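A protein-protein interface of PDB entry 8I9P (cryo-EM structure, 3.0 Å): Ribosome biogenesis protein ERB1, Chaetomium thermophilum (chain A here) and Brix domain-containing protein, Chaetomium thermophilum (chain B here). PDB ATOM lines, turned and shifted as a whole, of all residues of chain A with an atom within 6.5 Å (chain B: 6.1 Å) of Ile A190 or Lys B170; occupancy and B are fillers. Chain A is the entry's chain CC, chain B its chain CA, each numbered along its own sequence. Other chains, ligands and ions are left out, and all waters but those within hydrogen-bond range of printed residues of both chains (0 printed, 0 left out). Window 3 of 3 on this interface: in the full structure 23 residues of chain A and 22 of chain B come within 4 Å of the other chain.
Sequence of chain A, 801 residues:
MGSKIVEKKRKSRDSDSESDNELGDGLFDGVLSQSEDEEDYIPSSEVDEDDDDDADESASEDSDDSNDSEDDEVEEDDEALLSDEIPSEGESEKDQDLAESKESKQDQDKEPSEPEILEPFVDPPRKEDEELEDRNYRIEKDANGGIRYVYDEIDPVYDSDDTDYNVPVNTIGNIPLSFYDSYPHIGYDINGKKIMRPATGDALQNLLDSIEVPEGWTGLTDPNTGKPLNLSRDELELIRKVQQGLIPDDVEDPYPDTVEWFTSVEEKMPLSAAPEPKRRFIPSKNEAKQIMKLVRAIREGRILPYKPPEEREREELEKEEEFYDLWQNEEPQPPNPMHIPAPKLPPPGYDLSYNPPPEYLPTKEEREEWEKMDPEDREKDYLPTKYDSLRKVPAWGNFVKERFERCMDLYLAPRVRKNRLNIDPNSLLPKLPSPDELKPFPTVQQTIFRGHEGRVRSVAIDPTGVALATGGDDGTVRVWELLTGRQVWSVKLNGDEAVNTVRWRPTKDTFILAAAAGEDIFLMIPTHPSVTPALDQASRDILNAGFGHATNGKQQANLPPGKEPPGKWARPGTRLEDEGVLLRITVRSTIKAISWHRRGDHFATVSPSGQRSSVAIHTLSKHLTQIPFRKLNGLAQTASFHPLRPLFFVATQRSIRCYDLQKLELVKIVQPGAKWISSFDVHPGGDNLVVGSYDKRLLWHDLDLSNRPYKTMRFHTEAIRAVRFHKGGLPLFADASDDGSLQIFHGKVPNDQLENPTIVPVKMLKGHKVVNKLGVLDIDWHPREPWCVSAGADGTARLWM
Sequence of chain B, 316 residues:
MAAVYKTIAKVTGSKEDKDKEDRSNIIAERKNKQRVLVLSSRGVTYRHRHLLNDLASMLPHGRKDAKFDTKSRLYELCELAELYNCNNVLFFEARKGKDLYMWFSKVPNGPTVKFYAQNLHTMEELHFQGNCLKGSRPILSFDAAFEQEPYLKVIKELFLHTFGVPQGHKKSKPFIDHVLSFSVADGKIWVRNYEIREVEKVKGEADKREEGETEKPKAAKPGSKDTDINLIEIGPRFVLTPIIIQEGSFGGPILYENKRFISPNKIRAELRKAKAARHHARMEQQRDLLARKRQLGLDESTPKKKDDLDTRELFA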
ATOM      1  N   TYR A 165      12.223 -20.163 -13.752  1.00  0.00           N
ATOM      2  CA  TYR A 165      11.748 -21.204 -14.659  1.00  0.00           C
ATOM      3  C   TYR A 165      11.152 -20.609 -15.929  1.00  0.00           C
ATOM      4  O   TYR A 165      11.334 -21.156 -17.022  1.00  0.00           O
ATOM      5  CB  TYR A 165      10.728 -22.080 -13.932  1.00  0.00           C
ATOM      6  CG  TYR A 165       9.918 -23.003 -14.812  1.00  0.00           C
ATOM      7  CD1 TYR A 165      10.530 -23.964 -15.606  1.00  0.00           C
ATOM      8  CD2 TYR A 165       8.530 -22.924 -14.831  1.00  0.00           C
ATOM      9  CE1 TYR A 165       9.782 -24.812 -16.406  1.00  0.00           C
ATOM     10  CE2 TYR A 165       7.776 -23.766 -15.625  1.00  0.00           C
ATOM     11  CZ  TYR A 165       8.407 -24.707 -16.409  1.00  0.00           C
ATOM     12  OH  TYR A 165       7.656 -25.546 -17.199  1.00  0.00           O
ATOM     13  N   VAL A 167      11.612 -17.335 -17.691  1.00  0.00           N
ATOM     14  CA  VAL A 167      12.338 -16.083 -17.888  1.00  0.00           C
ATOM     15  C   VAL A 167      11.877 -15.472 -19.207  1.00  0.00           C
ATOM     16  O   VAL A 167      11.832 -16.173 -20.228  1.00  0.00           O
ATOM     17  CB  VAL A 167      13.857 -16.319 -17.851  1.00  0.00           C
ATOM     18  CG1 VAL A 167      14.600 -15.032 -18.179  1.00  0.00           C
ATOM     19  CG2 VAL A 167      14.298 -16.878 -16.509  1.00  0.00           C
ATOM     20  N   PRO A 168      11.505 -14.190 -19.231  1.00  0.00           N
ATOM     21  CA  PRO A 168      10.948 -13.595 -20.454  1.00  0.00           C
ATOM     22  C   PRO A 168      11.991 -13.441 -21.551  1.00  0.00           C
ATOM     23  O   PRO A 168      13.201 -13.530 -21.335  1.00  0.00           O
ATOM     24  CB  PRO A 168      10.436 -12.231 -19.979  1.00  0.00           C
ATOM     25  CG  PRO A 168      11.263 -11.924 -18.777  1.00  0.00           C
ATOM     26  CD  PRO A 168      11.488 -13.244 -18.103  1.00  0.00           C
ATOM     27  N   VAL A 169      11.490 -13.192 -22.760  1.00  0.00           N
ATOM     28  CA  VAL A 169      12.300 -13.103 -23.968  1.00  0.00           C
ATOM     29  C   VAL A 169      12.409 -11.659 -24.466  1.00  0.00           C
ATOM     30  O   VAL A 169      12.693 -11.425 -25.635  1.00  0.00           O
ATOM     31  CB  VAL A 169      11.749 -14.033 -25.068  1.00  0.00           C
ATOM     32  CG1 VAL A 169      12.520 -13.851 -26.368  1.00  0.00           C
ATOM     33  CG2 VAL A 169      11.794 -15.492 -24.616  1.00  0.00           C
ATOM     34  N   THR A 171      14.261  -9.360 -22.502  1.00  0.00           N
ATOM     35  CA  THR A 171      15.523  -8.991 -21.817  1.00  0.00           C
ATOM     36  C   THR A 171      15.519  -7.599 -21.171  1.00  0.00           C
ATOM     37  O   THR A 171      16.464  -6.822 -21.309  1.00  0.00           O
ATOM     38  CB  THR A 171      16.768  -9.193 -22.725  1.00  0.00           C
ATOM     39  OG1 THR A 171      17.964  -8.915 -21.983  1.00  0.00           O
ATOM     40  CG2 THR A 171      16.791  -8.364 -24.035  1.00  0.00           C
ATOM     41  N   TYR A 188      15.203  -5.447 -27.319  1.00  0.00           N
ATOM     42  CA  TYR A 188      15.913  -6.423 -28.135  1.00  0.00           C
ATOM     43  C   TYR A 188      15.681  -7.831 -27.578  1.00  0.00           C
ATOM     44  O   TYR A 188      14.813  -8.044 -26.728  1.00  0.00           O
ATOM     45  CB  TYR A 188      17.402  -6.067 -28.202  1.00  0.00           C
ATOM     46  CG  TYR A 188      17.753  -5.010 -29.224  1.00  0.00           C
ATOM     47  CD1 TYR A 188      17.967  -5.346 -30.555  1.00  0.00           C
ATOM     48  CD2 TYR A 188      17.874  -3.676 -28.859  1.00  0.00           C
ATOM     49  CE1 TYR A 188      18.292  -4.382 -31.493  1.00  0.00           C
ATOM     50  CE2 TYR A 188      18.197  -2.706 -29.787  1.00  0.00           C
ATOM     51  CZ  TYR A 188      18.405  -3.064 -31.102  1.00  0.00           C
ATOM     52  OH  TYR A 188      18.727  -2.098 -32.027  1.00  0.00           O
ATOM     53  N   ASP A 189      16.453  -8.804 -28.060  1.00  0.00           N
ATOM     54  CA  ASP A 189      16.434 -10.172 -27.555  1.00  0.00           C
ATOM     55  C   ASP A 189      17.884 -10.630 -27.397  1.00  0.00           C
ATOM     56  O   ASP A 189      18.812  -9.819 -27.448  1.00  0.00           O
ATOM     57  CB  ASP A 189      15.604 -11.083 -28.471  1.00  0.00           C
ATOM     58  CG  ASP A 189      16.348 -11.501 -29.728  1.00  0.00           C
ATOM     59  OD1 ASP A 189      17.092 -12.506 -29.685  1.00  0.00           O
ATOM     60  OD2 ASP A 189      16.188 -10.822 -30.760  1.00  0.00           O
ATOM     61  N   ILE A 190      18.072 -11.939 -27.191  1.00  0.00           N
ATOM     62  CA  ILE A 190      19.402 -12.488 -26.921  1.00  0.00           C
ATOM     63  C   ILE A 190      20.318 -12.317 -28.127  1.00  0.00           C
ATOM     64  O   ILE A 190      21.460 -11.856 -28.002  1.00  0.00           O
ATOM     65  CB  ILE A 190      19.288 -13.966 -26.500  1.00  0.00           C
ATOM     66  CG1 ILE A 190      18.879 -14.068 -25.033  1.00  0.00           C
ATOM     67  CG2 ILE A 190      20.600 -14.709 -26.716  1.00  0.00           C
ATOM     68  CD1 ILE A 190      19.695 -13.186 -24.120  1.00  0.00           C
ATOM     69  N   ASN A 191      19.829 -12.672 -29.316  1.00  0.00           N
ATOM     70  CA  ASN A 191      20.667 -12.590 -30.507  1.00  0.00           C
ATOM     71  C   ASN A 191      20.882 -11.147 -30.952  1.00  0.00           C
ATOM     72  O   ASN A 191      21.960 -10.806 -31.453  1.00  0.00           O
ATOM     73  CB  ASN A 191      20.054 -13.414 -31.637  1.00  0.00           C
ATOM     74  CG  ASN A 191      19.905 -14.876 -31.276  1.00  0.00           C
ATOM     75  OD1 ASN A 191      20.882 -15.550 -30.947  1.00  0.00           O
ATOM     76  ND2 ASN A 191      18.677 -15.378 -31.339  1.00  0.00           N
ATOM     77  N   GLY A 192      19.878 -10.289 -30.779  1.00  0.00           N
ATOM     78  CA  GLY A 192      20.022  -8.886 -31.116  1.00  0.00           C
ATOM     79  C   GLY A 192      19.019  -8.385 -32.136  1.00  0.00           C
ATOM     80  O   GLY A 192      19.224  -7.335 -32.753  1.00  0.00           O
ATOM     81  N   LYS A 193      17.935  -9.130 -32.328  1.00  0.00           N
ATOM     82  CA  LYS A 193      16.887  -8.738 -33.260  1.00  0.00           C
ATOM     83  C   LYS A 193      15.829  -7.900 -32.551  1.00  0.00           C
ATOM     84  O   LYS A 193      15.669  -7.975 -31.329  1.00  0.00           O
ATOM     85  CB  LYS A 193      16.242  -9.966 -33.910  1.00  0.00           C
ATOM     86  CG  LYS A 193      16.729 -10.268 -35.328  1.00  0.00           C
ATOM     87  CD  LYS A 193      18.230 -10.501 -35.415  1.00  0.00           C
ATOM     88  CE  LYS A 193      18.672 -11.689 -34.576  1.00  0.00           C
ATOM     89  NZ  LYS A 193      20.127 -11.965 -34.745  1.00  0.00           N
ATOM     90  N   ASN B  25      17.934 -23.746 -20.086  1.00  0.00           N
ATOM     91  CA  ASN B  25      17.952 -22.280 -20.130  1.00  0.00           C
ATOM     92  C   ASN B  25      19.182 -21.736 -20.856  1.00  0.00           C
ATOM     93  O   ASN B  25      19.631 -20.622 -20.581  1.00  0.00           O
ATOM     94  CB  ASN B  25      17.845 -21.666 -18.727  1.00  0.00           C
ATOM     95  CG  ASN B  25      16.787 -20.587 -18.643  1.00  0.00           C
ATOM     96  OD1 ASN B  25      16.214 -20.182 -19.655  1.00  0.00           O
ATOM     97  ND2 ASN B  25      16.522 -20.112 -17.432  1.00  0.00           N
ATOM     98  N   ILE B  26      19.732 -22.507 -21.793  1.00  0.00           N
ATOM     99  CA  ILE B  26      20.830 -22.065 -22.644  1.00  0.00           C
ATOM    100  C   ILE B  26      20.515 -22.478 -24.074  1.00  0.00           C
ATOM    101  O   ILE B  26      20.301 -23.664 -24.349  1.00  0.00           O
ATOM    102  CB  ILE B  26      22.183 -22.653 -22.195  1.00  0.00           C
ATOM    103  CG1 ILE B  26      22.638 -22.022 -20.879  1.00  0.00           C
ATOM    104  CG2 ILE B  26      23.244 -22.435 -23.262  1.00  0.00           C
ATOM    105  CD1 ILE B  26      23.807 -22.727 -20.239  1.00  0.00           C
ATOM    106  N   ILE B  27      20.482 -21.505 -24.981  1.00  0.00           N
ATOM    107  CA  ILE B  27      20.248 -21.746 -26.401  1.00  0.00           C
ATOM    108  C   ILE B  27      21.537 -21.441 -27.159  1.00  0.00           C
ATOM    109  O   ILE B  27      21.878 -20.273 -27.385  1.00  0.00           O
ATOM    110  CB  ILE B  27      19.062 -20.922 -26.930  1.00  0.00           C
ATOM    111  CG1 ILE B  27      19.006 -19.539 -26.270  1.00  0.00           C
ATOM    112  CG2 ILE B  27      17.756 -21.666 -26.705  1.00  0.00           C
ATOM    113  CD1 ILE B  27      17.972 -18.617 -26.877  1.00  0.00           C
ATOM    114  N   GLN B 167      26.461 -18.512 -23.104  1.00  0.00           N
ATOM    115  CA  GLN B 167      25.889 -18.021 -24.356  1.00  0.00           C
ATOM    116  C   GLN B 167      24.391 -17.748 -24.317  1.00  0.00           C
ATOM    117  O   GLN B 167      23.960 -16.595 -24.422  1.00  0.00           O
ATOM    118  CB  GLN B 167      26.171 -19.024 -25.480  1.00  0.00           C
ATOM    119  CG  GLN B 167      27.606 -19.498 -25.556  1.00  0.00           C
ATOM    120  CD  GLN B 167      28.386 -18.775 -26.634  1.00  0.00           C
ATOM    121  OE1 GLN B 167      29.353 -18.073 -26.348  1.00  0.00           O
ATOM    122  NE2 GLN B 167      27.971 -18.948 -27.882  1.00  0.00           N
ATOM    123  N   GLY B 168      23.593 -18.801 -24.163  1.00  0.00           N
ATOM    124  CA  GLY B 168      22.170 -18.709 -24.420  1.00  0.00           C
ATOM    125  C   GLY B 168      21.315 -18.476 -23.196  1.00  0.00           C
ATOM    126  O   GLY B 168      20.106 -18.724 -23.216  1.00  0.00           O
ATOM    127  N   HIS B 169      21.935 -18.002 -22.122  1.00  0.00           N
ATOM    128  CA  HIS B 169      21.199 -17.707 -20.904  1.00  0.00           C
ATOM    129  C   HIS B 169      20.387 -16.435 -21.117  1.00  0.00           C
ATOM    130  O   HIS B 169      20.949 -15.348 -21.263  1.00  0.00           O
ATOM    131  CB  HIS B 169      22.184 -17.543 -19.746  1.00  0.00           C
ATOM    132  CG  HIS B 169      21.582 -17.753 -18.393  1.00  0.00           C
ATOM    133  ND1 HIS B 169      20.590 -16.948 -17.880  1.00  0.00           N
ATOM    134  CD2 HIS B 169      21.850 -18.676 -17.440  1.00  0.00           C
ATOM    135  CE1 HIS B 169      20.266 -17.372 -16.672  1.00  0.00           C
ATOM    136  NE2 HIS B 169      21.015 -18.420 -16.381  1.00  0.00           N
ATOM    137  N   LYS B 170      19.066 -16.603 -21.251  1.00  0.00           N
ATOM    138  CA  LYS B 170      18.162 -15.479 -21.638  1.00  0.00           C
ATOM    139  C   LYS B 170      18.287 -14.231 -20.762  1.00  0.00           C
ATOM    140  O   LYS B 170      18.048 -13.130 -21.296  1.00  0.00           O
ATOM    141  CB  LYS B 170      16.710 -15.969 -21.615  1.00  0.00           C
ATOM    142  CG  LYS B 170      16.451 -17.259 -22.381  1.00  0.00           C
ATOM    143  CD  LYS B 170      15.039 -17.774 -22.221  1.00  0.00           C
ATOM    144  CE  LYS B 170      14.829 -19.130 -22.862  1.00  0.00           C
ATOM    145  NZ  LYS B 170      13.463 -19.647 -22.607  1.00  0.00           N
ATOM    146  N   LYS B 171      18.607 -14.374 -19.477  1.00  0.00           N
ATOM    147  CA  LYS B 171      18.607 -13.187 -18.633  1.00  0.00           C
ATOM    148  C   LYS B 171      19.791 -12.277 -18.927  1.00  0.00           C
ATOM    149  O   LYS B 171      19.957 -11.258 -18.251  1.00  0.00           O
ATOM    150  CB  LYS B 171      18.604 -13.575 -17.152  1.00  0.00           C
ATOM    151  CG  LYS B 171      17.914 -14.890 -16.853  1.00  0.00           C
ATOM    152  CD  LYS B 171      17.899 -15.188 -15.360  1.00  0.00           C
ATOM    153  CE  LYS B 171      17.479 -13.988 -14.525  1.00  0.00           C
ATOM    154  NZ  LYS B 171      15.998 -13.851 -14.453  1.00  0.00           N
ATOM    155  N   SER B 172      20.609 -12.622 -19.917  1.00  0.00           N
ATOM    156  CA  SER B 172      21.805 -11.867 -20.258  1.00  0.00           C
ATOM    157  C   SER B 172      21.481 -10.730 -21.219  1.00  0.00           C
ATOM    158  O   SER B 172      20.568 -10.829 -22.043  1.00  0.00           O
ATOM    159  CB  SER B 172      22.849 -12.783 -20.893  1.00  0.00           C
ATOM    160  OG  SER B 172      22.574 -12.973 -22.270  1.00  0.00           O
ATOM    161  N   LYS B 173      22.239  -9.646 -21.109  1.00  0.00           N
ATOM    162  CA  LYS B 173      22.134  -8.575 -22.084  1.00  0.00           C
ATOM    163  C   LYS B 173      22.889  -8.944 -23.359  1.00  0.00           C
ATOM    164  O   LYS B 173      23.933  -9.598 -23.306  1.00  0.00           O
ATOM    165  CB  LYS B 173      22.673  -7.271 -21.502  1.00  0.00           C
ATOM    166  CG  LYS B 173      21.851  -6.706 -20.362  1.00  0.00           C
ATOM    167  CD  LYS B 173      20.375  -6.646 -20.702  1.00  0.00           C
ATOM    168  CE  LYS B 173      19.531  -6.991 -19.491  1.00  0.00           C
ATOM    169  NZ  LYS B 173      19.797  -8.375 -19.020  1.00  0.00           N
ATOM    170  N   PRO B 174      22.384  -8.536 -24.524  1.00  0.00           N
ATOM    171  CA  PRO B 174      23.016  -8.931 -25.795  1.00  0.00           C
ATOM    172  C   PRO B 174      24.186  -8.067 -26.252  1.00  0.00           C
ATOM    173  O   PRO B 174      24.948  -8.524 -27.110  1.00  0.00           O
ATOM    174  CB  PRO B 174      21.855  -8.803 -26.785  1.00  0.00           C
ATOM    175  CG  PRO B 174      20.953  -7.765 -26.206  1.00  0.00           C
ATOM    176  CD  PRO B 174      21.242  -7.628 -24.741  1.00  0.00           C
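OG1 of Thr A171 is in hydrogen-bond range of O of Ser B172, 3.2 Å away.
O of His B169 is in hydrogen-bond range of OG of Ser B172, 3.0 Å away. NZ of Lys B173 lies within hydrogen-bond range of O of Lys B171 (3.0 Å). The backbone NH (N) of Asn A191 lies within hydrogen-bond range of the side-chain carboxylate (OD1) of Asp A189 (2.8 Å). The backbone NH (N) of Lys A193 is in hydrogen-bond range of the side-chain carboxylate (OD2) of Asp A189 (2.9 Å).
Hydrophobic or aromatic side chains of chain B within 4 Å of the printed part of chain A: Pro B174. Of the 11 printed residues of chain A, 4 touch a printed residue of chain B. Hydrophobic or aromatic side chains of chain A that line the printed part of chain B: Val A167 and Ile A190.
Of the printed residues of chain B, Thr A171 touches Ser B172 (3.2 Å) and Lys B173 (3.5 Å). Ile A190 touches four residues of chain B. Lys B170 touches just one residue of chain A: Ile A190. Of the printed residues of chain A, Lys B171 touches Val A167. Of the printed residues of chain A, Ser B172 touches Thr A171 and Ile A190. Printed residues of chain A within 4 Å of Lys B173: Thr A171. The nearest residue of chain A that does not touch Lys B170 is Val A167 (4.1 Å).
Val A167 touches Lys B171. CE of Lys B173 touches OG1 of Thr A171, 3.5 Å away. O of Asp A189 touches CG of Pro B174 (3.2 Å). Ile A190 touches His B169 (CD1 to O, 3.8 Å). CD1 of Ile A190 touches O of Lys B170, at 3.3 Å. O of Ser B172 touches CD1 of Ile A190 (3.3 Å). Pro B174 touches Ile A190.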
